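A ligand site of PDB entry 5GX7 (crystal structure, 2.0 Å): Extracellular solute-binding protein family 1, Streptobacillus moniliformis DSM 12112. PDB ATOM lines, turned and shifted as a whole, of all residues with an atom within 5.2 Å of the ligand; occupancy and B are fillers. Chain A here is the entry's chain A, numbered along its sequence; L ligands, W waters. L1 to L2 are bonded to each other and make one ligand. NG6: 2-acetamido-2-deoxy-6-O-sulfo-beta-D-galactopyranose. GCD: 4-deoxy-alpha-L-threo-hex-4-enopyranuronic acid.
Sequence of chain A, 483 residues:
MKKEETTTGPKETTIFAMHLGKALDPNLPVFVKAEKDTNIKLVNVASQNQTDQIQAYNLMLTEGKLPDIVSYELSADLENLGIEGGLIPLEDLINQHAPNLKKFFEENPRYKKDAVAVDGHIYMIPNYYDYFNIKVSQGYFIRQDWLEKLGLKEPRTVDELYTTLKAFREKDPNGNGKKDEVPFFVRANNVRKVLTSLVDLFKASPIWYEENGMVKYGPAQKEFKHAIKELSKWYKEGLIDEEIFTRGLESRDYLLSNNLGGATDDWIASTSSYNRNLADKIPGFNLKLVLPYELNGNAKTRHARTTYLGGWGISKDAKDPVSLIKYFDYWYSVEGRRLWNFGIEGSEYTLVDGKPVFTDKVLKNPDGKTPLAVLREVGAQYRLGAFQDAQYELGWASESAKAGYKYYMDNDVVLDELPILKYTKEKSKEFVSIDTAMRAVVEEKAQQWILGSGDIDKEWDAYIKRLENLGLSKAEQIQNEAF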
ATOM      1  N   HIS A  19     -20.918 -15.470  15.764  1.00  0.00           N
ATOM      2  CA  HIS A  19     -19.676 -15.708  15.073  1.00  0.00           C
ATOM      3  C   HIS A  19     -19.917 -16.829  14.089  1.00  0.00           C
ATOM      4  O   HIS A  19     -20.517 -17.839  14.469  1.00  0.00           O
ATOM      5  CB  HIS A  19     -18.539 -16.083  16.059  1.00  0.00           C
ATOM      6  CG  HIS A  19     -17.208 -16.276  15.379  1.00  0.00           C
ATOM      7  ND1 HIS A  19     -16.693 -15.353  14.490  1.00  0.00           N
ATOM      8  CD2 HIS A  19     -16.295 -17.288  15.470  1.00  0.00           C
ATOM      9  CE1 HIS A  19     -15.548 -15.798  14.015  1.00  0.00           C
ATOM     10  NE2 HIS A  19     -15.280 -16.979  14.589  1.00  0.00           N
ATOM     11  N   LEU A  20     -19.445 -16.637  12.861  1.00  0.00           N
ATOM     12  CA  LEU A  20     -19.540 -17.669  11.813  1.00  0.00           C
ATOM     13  C   LEU A  20     -20.977 -18.100  11.685  1.00  0.00           C
ATOM     14  O   LEU A  20     -21.290 -19.304  11.608  1.00  0.00           O
ATOM     15  CB  LEU A  20     -18.620 -18.861  12.099  1.00  0.00           C
ATOM     16  CG  LEU A  20     -17.134 -18.428  12.024  1.00  0.00           C
ATOM     17  CD1 LEU A  20     -16.229 -19.521  12.462  1.00  0.00           C
ATOM     18  CD2 LEU A  20     -16.787 -18.044  10.600  1.00  0.00           C
ATOM     19  N   GLU A  73     -18.155  -8.187  14.641  1.00  0.00           N
ATOM     20  CA  GLU A  73     -17.006  -8.461  13.782  1.00  0.00           C
ATOM     21  C   GLU A  73     -16.502  -7.203  13.088  1.00  0.00           C
ATOM     22  O   GLU A  73     -15.305  -7.111  12.760  1.00  0.00           O
ATOM     23  CB  GLU A  73     -17.364  -9.583  12.770  1.00  0.00           C
ATOM     24  CG  GLU A  73     -16.235  -9.958  11.830  1.00  0.00           C
ATOM     25  CD  GLU A  73     -16.398 -11.342  11.184  1.00  0.00           C
ATOM     26  OE1 GLU A  73     -16.923 -12.299  11.818  1.00  0.00           O
ATOM     27  OE2 GLU A  73     -15.950 -11.488  10.034  1.00  0.00           O
ATOM     28  N   ASN A 127     -10.465  -8.929  19.266  1.00  0.00           N
ATOM     29  CA  ASN A 127     -10.122 -10.348  19.301  1.00  0.00           C
ATOM     30  C   ASN A 127      -8.863 -10.528  18.471  1.00  0.00           C
ATOM     31  O   ASN A 127      -8.905 -10.476  17.253  1.00  0.00           O
ATOM     32  CB  ASN A 127     -11.251 -11.214  18.726  1.00  0.00           C
ATOM     33  CG  ASN A 127     -11.124 -12.652  19.148  1.00  0.00           C
ATOM     34  OD1 ASN A 127     -11.648 -13.040  20.197  1.00  0.00           O
ATOM     35  ND2 ASN A 127     -10.388 -13.442  18.379  1.00  0.00           N
ATOM     36  N   TYR A 129      -5.530 -12.021  16.684  1.00  0.00           N
ATOM     37  CA  TYR A 129      -4.802 -13.161  16.169  1.00  0.00           C
ATOM     38  C   TYR A 129      -3.398 -13.205  16.811  1.00  0.00           C
ATOM     39  O   TYR A 129      -2.888 -12.207  17.366  1.00  0.00           O
ATOM     40  CB  TYR A 129      -4.704 -13.059  14.639  1.00  0.00           C
ATOM     41  CG  TYR A 129      -5.975 -13.410  13.858  1.00  0.00           C
ATOM     42  CD1 TYR A 129      -6.451 -14.732  13.840  1.00  0.00           C
ATOM     43  CD2 TYR A 129      -6.661 -12.455  13.099  1.00  0.00           C
ATOM     44  CE1 TYR A 129      -7.615 -15.080  13.098  1.00  0.00           C
ATOM     45  CE2 TYR A 129      -7.816 -12.800  12.318  1.00  0.00           C
ATOM     46  CZ  TYR A 129      -8.276 -14.114  12.323  1.00  0.00           C
ATOM     47  OH  TYR A 129      -9.393 -14.476  11.604  1.00  0.00           O
ATOM     48  N   GLN A 138      -5.058 -17.546   3.947  1.00  0.00           N
ATOM     49  CA  GLN A 138      -5.588 -18.450   2.933  1.00  0.00           C
ATOM     50  C   GLN A 138      -4.508 -18.749   1.889  1.00  0.00           C
ATOM     51  O   GLN A 138      -3.631 -17.930   1.624  1.00  0.00           O
ATOM     52  CB  GLN A 138      -6.830 -17.868   2.252  1.00  0.00           C
ATOM     53  CG  GLN A 138      -7.977 -17.493   3.213  1.00  0.00           C
ATOM     54  CD  GLN A 138      -9.332 -17.268   2.485  1.00  0.00           C
ATOM     55  OE1 GLN A 138     -10.374 -17.246   3.117  1.00  0.00           O
ATOM     56  NE2 GLN A 138      -9.309 -17.100   1.160  1.00  0.00           N
ATOM     57  N   ARG A 187     -15.513 -21.224   0.559  1.00  0.00           N
ATOM     58  CA  ARG A 187     -16.165 -21.438   1.827  1.00  0.00           C
ATOM     59  C   ARG A 187     -16.291 -20.075   2.511  1.00  0.00           C
ATOM     60  O   ARG A 187     -15.279 -19.409   2.770  1.00  0.00           O
ATOM     61  CB  ARG A 187     -15.341 -22.412   2.691  1.00  0.00           C
ATOM     62  CG  ARG A 187     -15.966 -22.674   4.127  1.00  0.00           C
ATOM     63  CD  ARG A 187     -15.072 -23.678   4.942  1.00  0.00           C
ATOM     64  NE  ARG A 187     -13.766 -23.083   5.231  1.00  0.00           N
ATOM     65  CZ  ARG A 187     -13.373 -22.583   6.405  1.00  0.00           C
ATOM     66  NH1 ARG A 187     -14.143 -22.624   7.522  1.00  0.00           N
ATOM     67  NH2 ARG A 187     -12.170 -22.055   6.510  1.00  0.00           N
ATOM     68  N   ALA A 188     -17.528 -19.672   2.810  1.00  0.00           N
ATOM     69  CA  ALA A 188     -17.789 -18.303   3.239  1.00  0.00           C
ATOM     70  C   ALA A 188     -19.214 -18.247   3.785  1.00  0.00           C
ATOM     71  O   ALA A 188     -20.082 -19.070   3.442  1.00  0.00           O
ATOM     72  CB  ALA A 188     -17.644 -17.274   2.073  1.00  0.00           C
ATOM     73  N   ASN A 189     -19.450 -17.270   4.633  1.00  0.00           N
ATOM     74  CA  ASN A 189     -20.820 -17.155   5.102  1.00  0.00           C
ATOM     75  C   ASN A 189     -21.484 -15.842   4.727  1.00  0.00           C
ATOM     76  O   ASN A 189     -22.612 -15.601   5.179  1.00  0.00           O
ATOM     77  CB  ASN A 189     -20.883 -17.337   6.629  1.00  0.00           C
ATOM     78  CG  ASN A 189     -20.250 -16.189   7.384  1.00  0.00           C
ATOM     79  OD1 ASN A 189     -19.159 -15.704   7.029  1.00  0.00           O
ATOM     80  ND2 ASN A 189     -20.953 -15.690   8.395  1.00  0.00           N
ATOM     81  N   LYS A 193     -17.192 -12.380   1.745  1.00  0.00           N
ATOM     82  CA  LYS A 193     -16.222 -13.465   1.900  1.00  0.00           C
ATOM     83  C   LYS A 193     -16.259 -14.436   0.722  1.00  0.00           C
ATOM     84  O   LYS A 193     -15.226 -15.068   0.430  1.00  0.00           O
ATOM     85  CB  LYS A 193     -16.447 -14.211   3.222  1.00  0.00           C
ATOM     86  CG  LYS A 193     -16.077 -13.271   4.405  1.00  0.00           C
ATOM     87  CD  LYS A 193     -16.457 -13.895   5.744  1.00  0.00           C
ATOM     88  CE  LYS A 193     -16.014 -13.037   6.948  1.00  0.00           C
ATOM     89  NZ  LYS A 193     -17.032 -12.203   7.634  1.00  0.00           N
ATOM     90  N   LEU A 249     -21.170 -22.337   4.991  1.00  0.00           N
ATOM     91  CA  LEU A 249     -19.875 -22.733   5.569  1.00  0.00           C
ATOM     92  C   LEU A 249     -19.581 -24.209   5.506  1.00  0.00           C
ATOM     93  O   LEU A 249     -18.433 -24.595   5.742  1.00  0.00           O
ATOM     94  CB  LEU A 249     -19.769 -22.252   7.019  1.00  0.00           C
ATOM     95  CG  LEU A 249     -19.649 -20.736   7.195  1.00  0.00           C
ATOM     96  CD1 LEU A 249     -19.751 -20.325   8.691  1.00  0.00           C
ATOM     97  CD2 LEU A 249     -18.296 -20.311   6.678  1.00  0.00           C
ATOM     98  N   ARG A 252     -17.090 -26.694   1.897  1.00  0.00           N
ATOM     99  CA  ARG A 252     -15.834 -27.435   1.781  1.00  0.00           C
ATOM    100  C   ARG A 252     -15.990 -28.862   2.281  1.00  0.00           C
ATOM    101  O   ARG A 252     -15.547 -29.836   1.618  1.00  0.00           O
ATOM    102  CB  ARG A 252     -14.717 -26.714   2.569  1.00  0.00           C
ATOM    103  CG  ARG A 252     -13.320 -27.452   2.541  1.00  0.00           C
ATOM    104  CD  ARG A 252     -12.282 -26.589   3.348  1.00  0.00           C
ATOM    105  NE  ARG A 252     -12.697 -26.420   4.754  1.00  0.00           N
ATOM    106  CZ  ARG A 252     -11.983 -25.786   5.697  1.00  0.00           C
ATOM    107  NH1 ARG A 252     -10.804 -25.270   5.392  1.00  0.00           N
ATOM    108  NH2 ARG A 252     -12.413 -25.709   6.990  1.00  0.00           N
ATOM    109  N   ASP A 266      -8.464 -21.039   0.479  1.00  0.00           N
ATOM    110  CA  ASP A 266      -9.012 -21.119   1.834  1.00  0.00           C
ATOM    111  C   ASP A 266      -7.886 -21.176   2.882  1.00  0.00           C
ATOM    112  O   ASP A 266      -6.718 -21.433   2.561  1.00  0.00           O
ATOM    113  CB  ASP A 266      -9.909 -22.355   1.968  1.00  0.00           C
ATOM    114  CG  ASP A 266     -11.037 -22.212   2.983  1.00  0.00           C
ATOM    115  OD1 ASP A 266     -11.060 -21.244   3.814  1.00  0.00           O
ATOM    116  OD2 ASP A 266     -11.868 -23.172   2.992  1.00  0.00           O
ATOM    117  N   TRP A 267      -8.266 -21.062   4.170  1.00  0.00           N
ATOM    118  CA  TRP A 267      -7.283 -21.036   5.257  1.00  0.00           C
ATOM    119  C   TRP A 267      -6.390 -22.270   5.198  1.00  0.00           C
ATOM    120  O   TRP A 267      -6.887 -23.399   5.010  1.00  0.00           O
ATOM    121  CB  TRP A 267      -8.003 -21.020   6.606  1.00  0.00           C
ATOM    122  CG  TRP A 267      -8.594 -19.621   6.872  1.00  0.00           C
ATOM    123  CD1 TRP A 267      -9.736 -19.043   6.300  1.00  0.00           C
ATOM    124  CD2 TRP A 267      -8.048 -18.655   7.718  1.00  0.00           C
ATOM    125  NE1 TRP A 267      -9.898 -17.747   6.764  1.00  0.00           N
ATOM    126  CE2 TRP A 267      -8.865 -17.487   7.639  1.00  0.00           C
ATOM    127  CE3 TRP A 267      -6.884 -18.618   8.483  1.00  0.00           C
ATOM    128  CZ2 TRP A 267      -8.586 -16.335   8.353  1.00  0.00           C
ATOM    129  CZ3 TRP A 267      -6.622 -17.483   9.219  1.00  0.00           C
ATOM    130  CH2 TRP A 267      -7.458 -16.345   9.134  1.00  0.00           C
ATOM    131  N   ILE A 268      -5.108 -22.060   5.406  1.00  0.00           N
ATOM    132  CA  ILE A 268      -4.158 -23.110   5.085  1.00  0.00           C
ATOM    133  C   ILE A 268      -4.264 -24.285   6.066  1.00  0.00           C
ATOM    134  O   ILE A 268      -4.312 -25.460   5.645  1.00  0.00           O
ATOM    135  CB  ILE A 268      -2.732 -22.535   5.007  1.00  0.00           C
ATOM    136  CG1 ILE A 268      -2.582 -21.836   3.640  1.00  0.00           C
ATOM    137  CG2 ILE A 268      -1.644 -23.652   5.127  1.00  0.00           C
ATOM    138  CD1 ILE A 268      -1.386 -20.831   3.633  1.00  0.00           C
ATOM    139  N   ALA A 269      -4.262 -24.012   7.385  1.00  0.00           N
ATOM    140  CA  ALA A 269      -4.207 -25.150   8.309  1.00  0.00           C
ATOM    141  C   ALA A 269      -5.461 -26.037   8.174  1.00  0.00           C
ATOM    142  O   ALA A 269      -5.359 -27.263   8.023  1.00  0.00           O
ATOM    143  CB  ALA A 269      -4.021 -24.672   9.756  1.00  0.00           C
ATOM    144  N   SER A 270      -6.651 -25.450   8.223  1.00  0.00           N
ATOM    145  CA  SER A 270      -7.828 -26.327   8.167  1.00  0.00           C
ATOM    146  C   SER A 270      -8.024 -26.962   6.784  1.00  0.00           C
ATOM    147  O   SER A 270      -8.516 -28.090   6.676  1.00  0.00           O
ATOM    148  CB  SER A 270      -9.099 -25.561   8.591  1.00  0.00           C
ATOM    149  OG  SER A 270      -9.350 -24.485   7.722  1.00  0.00           O
ATOM    150  N   THR A 271      -7.659 -26.281   5.714  1.00  0.00           N
ATOM    151  CA  THR A 271      -7.810 -26.927   4.392  1.00  0.00           C
ATOM    152  C   THR A 271      -6.791 -28.072   4.223  1.00  0.00           C
ATOM    153  O   THR A 271      -7.127 -29.116   3.644  1.00  0.00           O
ATOM    154  CB  THR A 271      -7.663 -25.916   3.227  1.00  0.00           C
ATOM    155  OG1 THR A 271      -8.565 -24.797   3.435  1.00  0.00           O
ATOM    156  CG2 THR A 271      -8.050 -26.619   1.838  1.00  0.00           C
ATOM    157  N   ARG A 305      -3.232 -12.613   7.336  1.00  0.00           N
ATOM    158  CA  ARG A 305      -3.960 -12.438   8.575  1.00  0.00           C
ATOM    159  C   ARG A 305      -3.896 -10.958   8.968  1.00  0.00           C
ATOM    160  O   ARG A 305      -2.934 -10.273   8.651  1.00  0.00           O
ATOM    161  CB  ARG A 305      -3.343 -13.388   9.633  1.00  0.00           C
ATOM    162  CG  ARG A 305      -4.319 -14.027  10.563  1.00  0.00           C
ATOM    163  CD  ARG A 305      -3.703 -15.096  11.453  1.00  0.00           C
ATOM    164  NE  ARG A 305      -3.417 -16.316  10.718  1.00  0.00           N
ATOM    165  CZ  ARG A 305      -3.531 -17.537  11.228  1.00  0.00           C
ATOM    166  NH1 ARG A 305      -3.924 -17.710  12.488  1.00  0.00           N
ATOM    167  NH2 ARG A 305      -3.346 -18.604  10.442  1.00  0.00           N
ATOM    168  N   LEU A 309      -9.515  -9.270  14.605  1.00  0.00           N
ATOM    169  CA  LEU A 309     -10.823  -9.297  13.902  1.00  0.00           C
ATOM    170  C   LEU A 309     -11.875  -8.951  14.939  1.00  0.00           C
ATOM    171  O   LEU A 309     -12.010  -9.692  15.932  1.00  0.00           O
ATOM    172  CB  LEU A 309     -11.125 -10.684  13.301  1.00  0.00           C
ATOM    173  CG  LEU A 309     -12.472 -10.957  12.582  1.00  0.00           C
ATOM    174  CD1 LEU A 309     -12.570 -10.156  11.264  1.00  0.00           C
ATOM    175  CD2 LEU A 309     -12.630 -12.447  12.334  1.00  0.00           C
ATOM    176  N   LEU A 372     -10.276 -27.928  13.924  1.00  0.00           N
ATOM    177  CA  LEU A 372     -10.858 -26.632  14.278  1.00  0.00           C
ATOM    178  C   LEU A 372     -12.364 -26.730  14.425  1.00  0.00           C
ATOM    179  O   LEU A 372     -12.946 -26.157  15.352  1.00  0.00           O
ATOM    180  CB  LEU A 372     -10.458 -25.559  13.233  1.00  0.00           C
ATOM    181  CG  LEU A 372     -10.963 -24.136  13.527  1.00  0.00           C
ATOM    182  CD1 LEU A 372     -10.706 -23.618  14.931  1.00  0.00           C
ATOM    183  CD2 LEU A 372     -10.364 -23.112  12.548  1.00  0.00           C
ATOM    184  N   ARG A 376     -14.436 -25.663  17.700  1.00  0.00           N
ATOM    185  CA  ARG A 376     -15.497 -24.682  17.742  1.00  0.00           C
ATOM    186  C   ARG A 376     -16.761 -25.264  18.336  1.00  0.00           C
ATOM    187  O   ARG A 376     -17.539 -24.525  18.937  1.00  0.00           O
ATOM    188  CB  ARG A 376     -15.816 -24.107  16.332  1.00  0.00           C
ATOM    189  CG  ARG A 376     -14.655 -23.364  15.630  1.00  0.00           C
ATOM    190  CD  ARG A 376     -15.124 -22.531  14.416  1.00  0.00           C
ATOM    191  NE  ARG A 376     -14.016 -21.809  13.838  1.00  0.00           N
ATOM    192  CZ  ARG A 376     -13.482 -20.698  14.344  1.00  0.00           C
ATOM    193  NH1 ARG A 376     -14.014 -20.096  15.447  1.00  0.00           N
ATOM    194  NH2 ARG A 376     -12.445 -20.142  13.701  1.00  0.00           N
ATOM    195  N   GLN A 381     -12.091 -20.978  20.404  1.00  0.00           N
ATOM    196  CA  GLN A 381     -11.900 -20.124  19.210  1.00  0.00           C
ATOM    197  C   GLN A 381     -13.142 -19.236  18.858  1.00  0.00           C
ATOM    198  O   GLN A 381     -13.301 -18.801  17.700  1.00  0.00           O
ATOM    199  CB  GLN A 381     -11.514 -20.963  17.977  1.00  0.00           C
ATOM    200  CG  GLN A 381     -10.144 -21.652  18.208  1.00  0.00           C
ATOM    201  CD  GLN A 381      -9.042 -20.608  18.437  1.00  0.00           C
ATOM    202  OE1 GLN A 381      -8.954 -19.621  17.705  1.00  0.00           O
ATOM    203  NE2 GLN A 381      -8.162 -20.851  19.405  1.00  0.00           N
ATOM    204  N   ARG A 383     -14.852 -16.080  18.427  1.00  0.00           N
ATOM    205  CA  ARG A 383     -14.414 -14.702  18.296  1.00  0.00           C
ATOM    206  C   ARG A 383     -15.170 -13.783  19.231  1.00  0.00           C
ATOM    207  O   ARG A 383     -16.409 -13.665  19.171  1.00  0.00           O
ATOM    208  CB  ARG A 383     -14.612 -14.254  16.836  1.00  0.00           C
ATOM    209  CG  ARG A 383     -13.778 -12.990  16.437  1.00  0.00           C
ATOM    210  CD  ARG A 383     -14.455 -11.678  16.753  1.00  0.00           C
ATOM    211  NE  ARG A 383     -15.859 -11.566  16.374  1.00  0.00           N
ATOM    212  CZ  ARG A 383     -16.701 -10.858  17.120  1.00  0.00           C
ATOM    213  NH1 ARG A 383     -16.202 -10.240  18.195  1.00  0.00           N
ATOM    214  NH2 ARG A 383     -18.017 -10.742  16.801  1.00  0.00           N
ATOM    215  N   GLN A 388      -5.637 -14.922  20.529  1.00  0.00           N
ATOM    216  CA  GLN A 388      -5.346 -16.240  20.010  1.00  0.00           C
ATOM    217  C   GLN A 388      -3.895 -16.628  20.394  1.00  0.00           C
ATOM    218  O   GLN A 388      -3.033 -15.760  20.578  1.00  0.00           O
ATOM    219  CB  GLN A 388      -5.513 -16.260  18.475  1.00  0.00           C
ATOM    220  CG  GLN A 388      -5.277 -17.672  17.902  1.00  0.00           C
ATOM    221  CD  GLN A 388      -5.642 -17.692  16.409  1.00  0.00           C
ATOM    222  OE1 GLN A 388      -4.866 -17.235  15.555  1.00  0.00           O
ATOM    223  NE2 GLN A 388      -6.888 -18.135  16.100  1.00  0.00           N
ATOM    224  N   TYR A 392      -2.041 -23.184  19.761  1.00  0.00           N
ATOM    225  CA  TYR A 392      -3.215 -24.014  19.572  1.00  0.00           C
ATOM    226  C   TYR A 392      -3.272 -24.486  18.127  1.00  0.00           C
ATOM    227  O   TYR A 392      -3.550 -25.643  17.832  1.00  0.00           O
ATOM    228  CB  TYR A 392      -4.565 -23.283  19.966  1.00  0.00           C
ATOM    229  CG  TYR A 392      -5.366 -22.790  18.752  1.00  0.00           C
ATOM    230  CD1 TYR A 392      -5.034 -21.625  18.079  1.00  0.00           C
ATOM    231  CD2 TYR A 392      -6.277 -23.635  18.164  1.00  0.00           C
ATOM    232  CE1 TYR A 392      -5.786 -21.245  16.868  1.00  0.00           C
ATOM    233  CE2 TYR A 392      -6.979 -23.334  17.019  1.00  0.00           C
ATOM    234  CZ  TYR A 392      -6.761 -22.178  16.377  1.00  0.00           C
ATOM    235  OH  TYR A 392      -7.629 -22.241  15.271  1.00  0.00           O
ATOM    236  N   GLU A 393      -2.958 -23.580  17.201  1.00  0.00           N
ATOM    237  CA  GLU A 393      -2.986 -23.921  15.786  1.00  0.00           C
ATOM    238  C   GLU A 393      -1.876 -24.913  15.444  1.00  0.00           C
ATOM    239  O   GLU A 393      -2.122 -25.932  14.774  1.00  0.00           O
ATOM    240  CB  GLU A 393      -2.874 -22.612  14.946  1.00  0.00           C
ATOM    241  CG  GLU A 393      -3.286 -22.763  13.512  1.00  0.00           C
ATOM    242  CD  GLU A 393      -3.383 -21.446  12.733  1.00  0.00           C
ATOM    243  OE1 GLU A 393      -3.019 -21.461  11.530  1.00  0.00           O
ATOM    244  OE2 GLU A 393      -3.818 -20.427  13.306  1.00  0.00           O
ATOM    245  N   TRP A 396      -2.701 -28.792  16.257  1.00  0.00           N
ATOM    246  CA  TRP A 396      -3.453 -29.645  15.356  1.00  0.00           C
ATOM    247  C   TRP A 396      -3.049 -29.513  13.879  1.00  0.00           C
ATOM    248  O   TRP A 396      -3.436 -30.359  13.066  1.00  0.00           O
ATOM    249  CB  TRP A 396      -4.955 -29.402  15.482  1.00  0.00           C
ATOM    250  CG  TRP A 396      -5.427 -27.984  15.227  1.00  0.00           C
ATOM    251  CD1 TRP A 396      -5.644 -27.005  16.159  1.00  0.00           C
ATOM    252  CD2 TRP A 396      -5.793 -27.446  13.956  1.00  0.00           C
ATOM    253  NE1 TRP A 396      -6.144 -25.863  15.530  1.00  0.00           N
ATOM    254  CE2 TRP A 396      -6.218 -26.114  14.173  1.00  0.00           C
ATOM    255  CE3 TRP A 396      -5.807 -27.958  12.636  1.00  0.00           C
ATOM    256  CZ2 TRP A 396      -6.634 -25.264  13.119  1.00  0.00           C
ATOM    257  CZ3 TRP A 396      -6.243 -27.076  11.563  1.00  0.00           C
ATOM    258  CH2 TRP A 396      -6.626 -25.772  11.829  1.00  0.00           C
HETATM  259  C1  NG6 L   1     -12.837 -16.119  10.635  1.00  0.00           C
HETATM  260  C2  NG6 L   1     -12.118 -17.023  11.639  1.00  0.00           C
HETATM  261  C3  NG6 L   1     -11.083 -17.865  10.911  1.00  0.00           C
HETATM  262  C4  NG6 L   1     -11.746 -18.678   9.812  1.00  0.00           C
HETATM  263  C5  NG6 L   1     -12.558 -17.728   8.931  1.00  0.00           C
HETATM  264  C6  NG6 L   1     -13.316 -18.506   7.896  1.00  0.00           C
HETATM  265  C7  NG6 L   1     -11.687 -16.209  13.974  1.00  0.00           C
HETATM  266  C8  NG6 L   1     -10.947 -15.146  14.762  1.00  0.00           C
HETATM  267  N2  NG6 L   1     -11.393 -16.231  12.653  1.00  0.00           N
HETATM  268  O1  NG6 L   1     -13.844 -15.481  11.396  1.00  0.00           O
HETATM  269  O3  NG6 L   1     -10.573 -18.747  11.870  1.00  0.00           O
HETATM  270  O4  NG6 L   1     -12.671 -19.619  10.381  1.00  0.00           O
HETATM  271  O5  NG6 L   1     -13.524 -16.983   9.705  1.00  0.00           O
HETATM  272  O6  NG6 L   1     -13.882 -17.395   7.210  1.00  0.00           O
HETATM  273  O7  NG6 L   1     -12.468 -16.999  14.534  1.00  0.00           O
HETATM  274  S   NG6 L   1     -13.984 -17.384   5.732  1.00  0.00           S
HETATM  275  O1S NG6 L   1     -14.219 -16.085   5.172  1.00  0.00           O
HETATM  276  O2S NG6 L   1     -15.301 -18.390   5.802  1.00  0.00           O
HETATM  277  O3S NG6 L   1     -12.747 -17.884   5.180  1.00  0.00           O
HETATM  278  C1  GCD L   2      -9.237 -19.182  11.556  1.00  0.00           C
HETATM  279  C2  GCD L   2      -8.548 -19.478  12.906  1.00  0.00           C
HETATM  280  C3  GCD L   2      -7.101 -19.849  12.594  1.00  0.00           C
HETATM  281  C4  GCD L   2      -7.035 -20.920  11.475  1.00  0.00           C
HETATM  282  C5  GCD L   2      -8.111 -21.174  10.702  1.00  0.00           C
HETATM  283  C6  GCD L   2      -8.192 -22.236   9.698  1.00  0.00           C
HETATM  284  O2  GCD L   2      -8.533 -18.218  13.606  1.00  0.00           O
HETATM  285  O3  GCD L   2      -6.445 -20.326  13.809  1.00  0.00           O
HETATM  286  O5  GCD L   2      -9.306 -20.378  10.815  1.00  0.00           O
HETATM  287  O6A GCD L   2      -9.330 -22.423   9.134  1.00  0.00           O
HETATM  288  O6B GCD L   2      -7.155 -22.895   9.429  1.00  0.00           O
HETATM  289  O   HOH W   1     -10.260 -18.567  15.712  1.00  0.00           O
HETATM  290  O   HOH W   2     -11.822 -21.995   9.515  1.00  0.00           O
HETATM  291  O   HOH W   3     -16.294 -15.576   8.638  1.00  0.00           O
HETATM  292  O   HOH W   4     -13.596 -16.472   2.082  1.00  0.00           O
HETATM  293  O   HOH W   5     -12.590 -19.008   2.967  1.00  0.00           O
HETATM  294  O   HOH W   6      -4.765 -21.551   9.003  1.00  0.00           O
HETATM  295  O   HOH W   7      -8.899 -12.949  15.836  1.00  0.00           O
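The backbone NH of Ser 270 sits at hydrogen-bond distance from an oxygen (O6B) of GCD L2 (2.9 Å).
O6A of GCD L2 sits at hydrogen-bond distance from OG of Ser 270, 2.5 Å away.
An oxygen (O3) of GCD L2 sits at hydrogen-bond distance from the side-chain carboxylate (OE2) of Glu 393, 2.7 Å away.
The side-chain hydroxyl of Tyr 392 sits at hydrogen-bond distance from an oxygen (O3) of GCD L2, 2.7 Å away.
A ring nitrogen (NE2) of His 19 lies within hydrogen-bond range of an oxygen (O7) of NG6 L1 (2.8 Å).
OH of Tyr 129 lies within hydrogen-bond range of N2 of NG6 L1 (2.9 Å).
The guanidinium group of Arg 376 is in hydrogen-bond range of an oxygen (O3) of NG6 L1, at 3.0 Å.
An oxygen (O2) of GCD L2 sits at hydrogen-bond distance from the side-chain amide nitrogen of Gln 388 (3.0 Å).
The indole nitrogen of Trp 267 is in hydrogen-bond range of an oxygen (O3S) of NG6 L1 (3.3 Å).
The guanidinium group (NH2) of Arg 187 lies within salt-bridge range of an oxygen (O6A) of GCD L2 (3.9 Å).
The side-chain amide oxygen (OE1) of Gln 138 sits close to an oxygen (O3S) of NG6 L1, 3.2 Å away.
The side-chain hydroxyl (OG) of Ser 270 sits at hydrogen-bond distance from the guanidinium group (NH1) of Arg 252 (2.9 Å).
OE2 of Glu 393 is in salt-bridge range of NH1 of Arg 305.
O of Tyr 392 sits close to NE1 of Trp 396 (3.5 Å).
NH1 of Arg 376 is in hydrogen-bond range of O of Gln 381, 2.7 Å away.
The side-chain amide nitrogen of Gln 388 is in hydrogen-bond range of the side-chain amide oxygen of Gln 381 (3.0 Å).
OE1 of Gln 388 lies within hydrogen-bond range of NH1 of Arg 305, at 3.2 Å.
OE2 of Glu 73 lies within salt-bridge range of NZ of Lys 193 (2.7 Å).
The guanidinium group (NE) of Arg 187 lies within salt-bridge range of the side-chain carboxylate (OD2) of Asp 266 (2.9 Å).
Merely in contact with the ligand: Lys 193, Leu 309, Leu 372, Leu 20, Ala 188, Ala 269, Leu 249, Gln 381, Trp 396, Arg 305 and Arg 383.
Hydrophobic or aromatic side chains that line the ligand: His 19, Leu 20, Tyr 129, Leu 249, Trp 267, Ala 269, Leu 309, Leu 372, Tyr 392 and Trp 396.
21 residues have an atom within 4 Å of the ligand: His 19, Leu 20, Tyr 129, Gln 138, Arg 187, Ala 188, Lys 193, Leu 249, Trp 267, Ala 269, Ser 270, Arg 305, Leu 309, Leu 372, Arg 376, Gln 381, Arg 383, Gln 388, Tyr 392, Glu 393 and Trp 396.
The nearest printed residue that does not touch the ligand is Asp 266 (4.0002 Å).
Water W2 lies within hydrogen-bond range of O6A of GCD L2 (2.6 Å) and NH2 of Arg 187 (3.0 Å).
Water W1 lies within hydrogen-bond range of the side-chain amide oxygen of Gln 381 (2.6 Å), an oxygen (O2) of GCD L2 (2.7 Å), the guanidinium group of Arg 376 (3.4 Å) and the side-chain amide nitrogen of Gln 388 (3.4 Å).
Water W6 lies within hydrogen-bond range of an oxygen (O6B) of GCD L2 (2.8 Å), the backbone NH (N) of Ala 269 (3.0 Å) and the side-chain carboxylate (OE1) of Glu 393 (3.1 Å).
Water W3 lies within hydrogen-bond range of O5 of NG6 L1 (3.3 Å) and OD1 of Asn 189 (3.3 Å).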
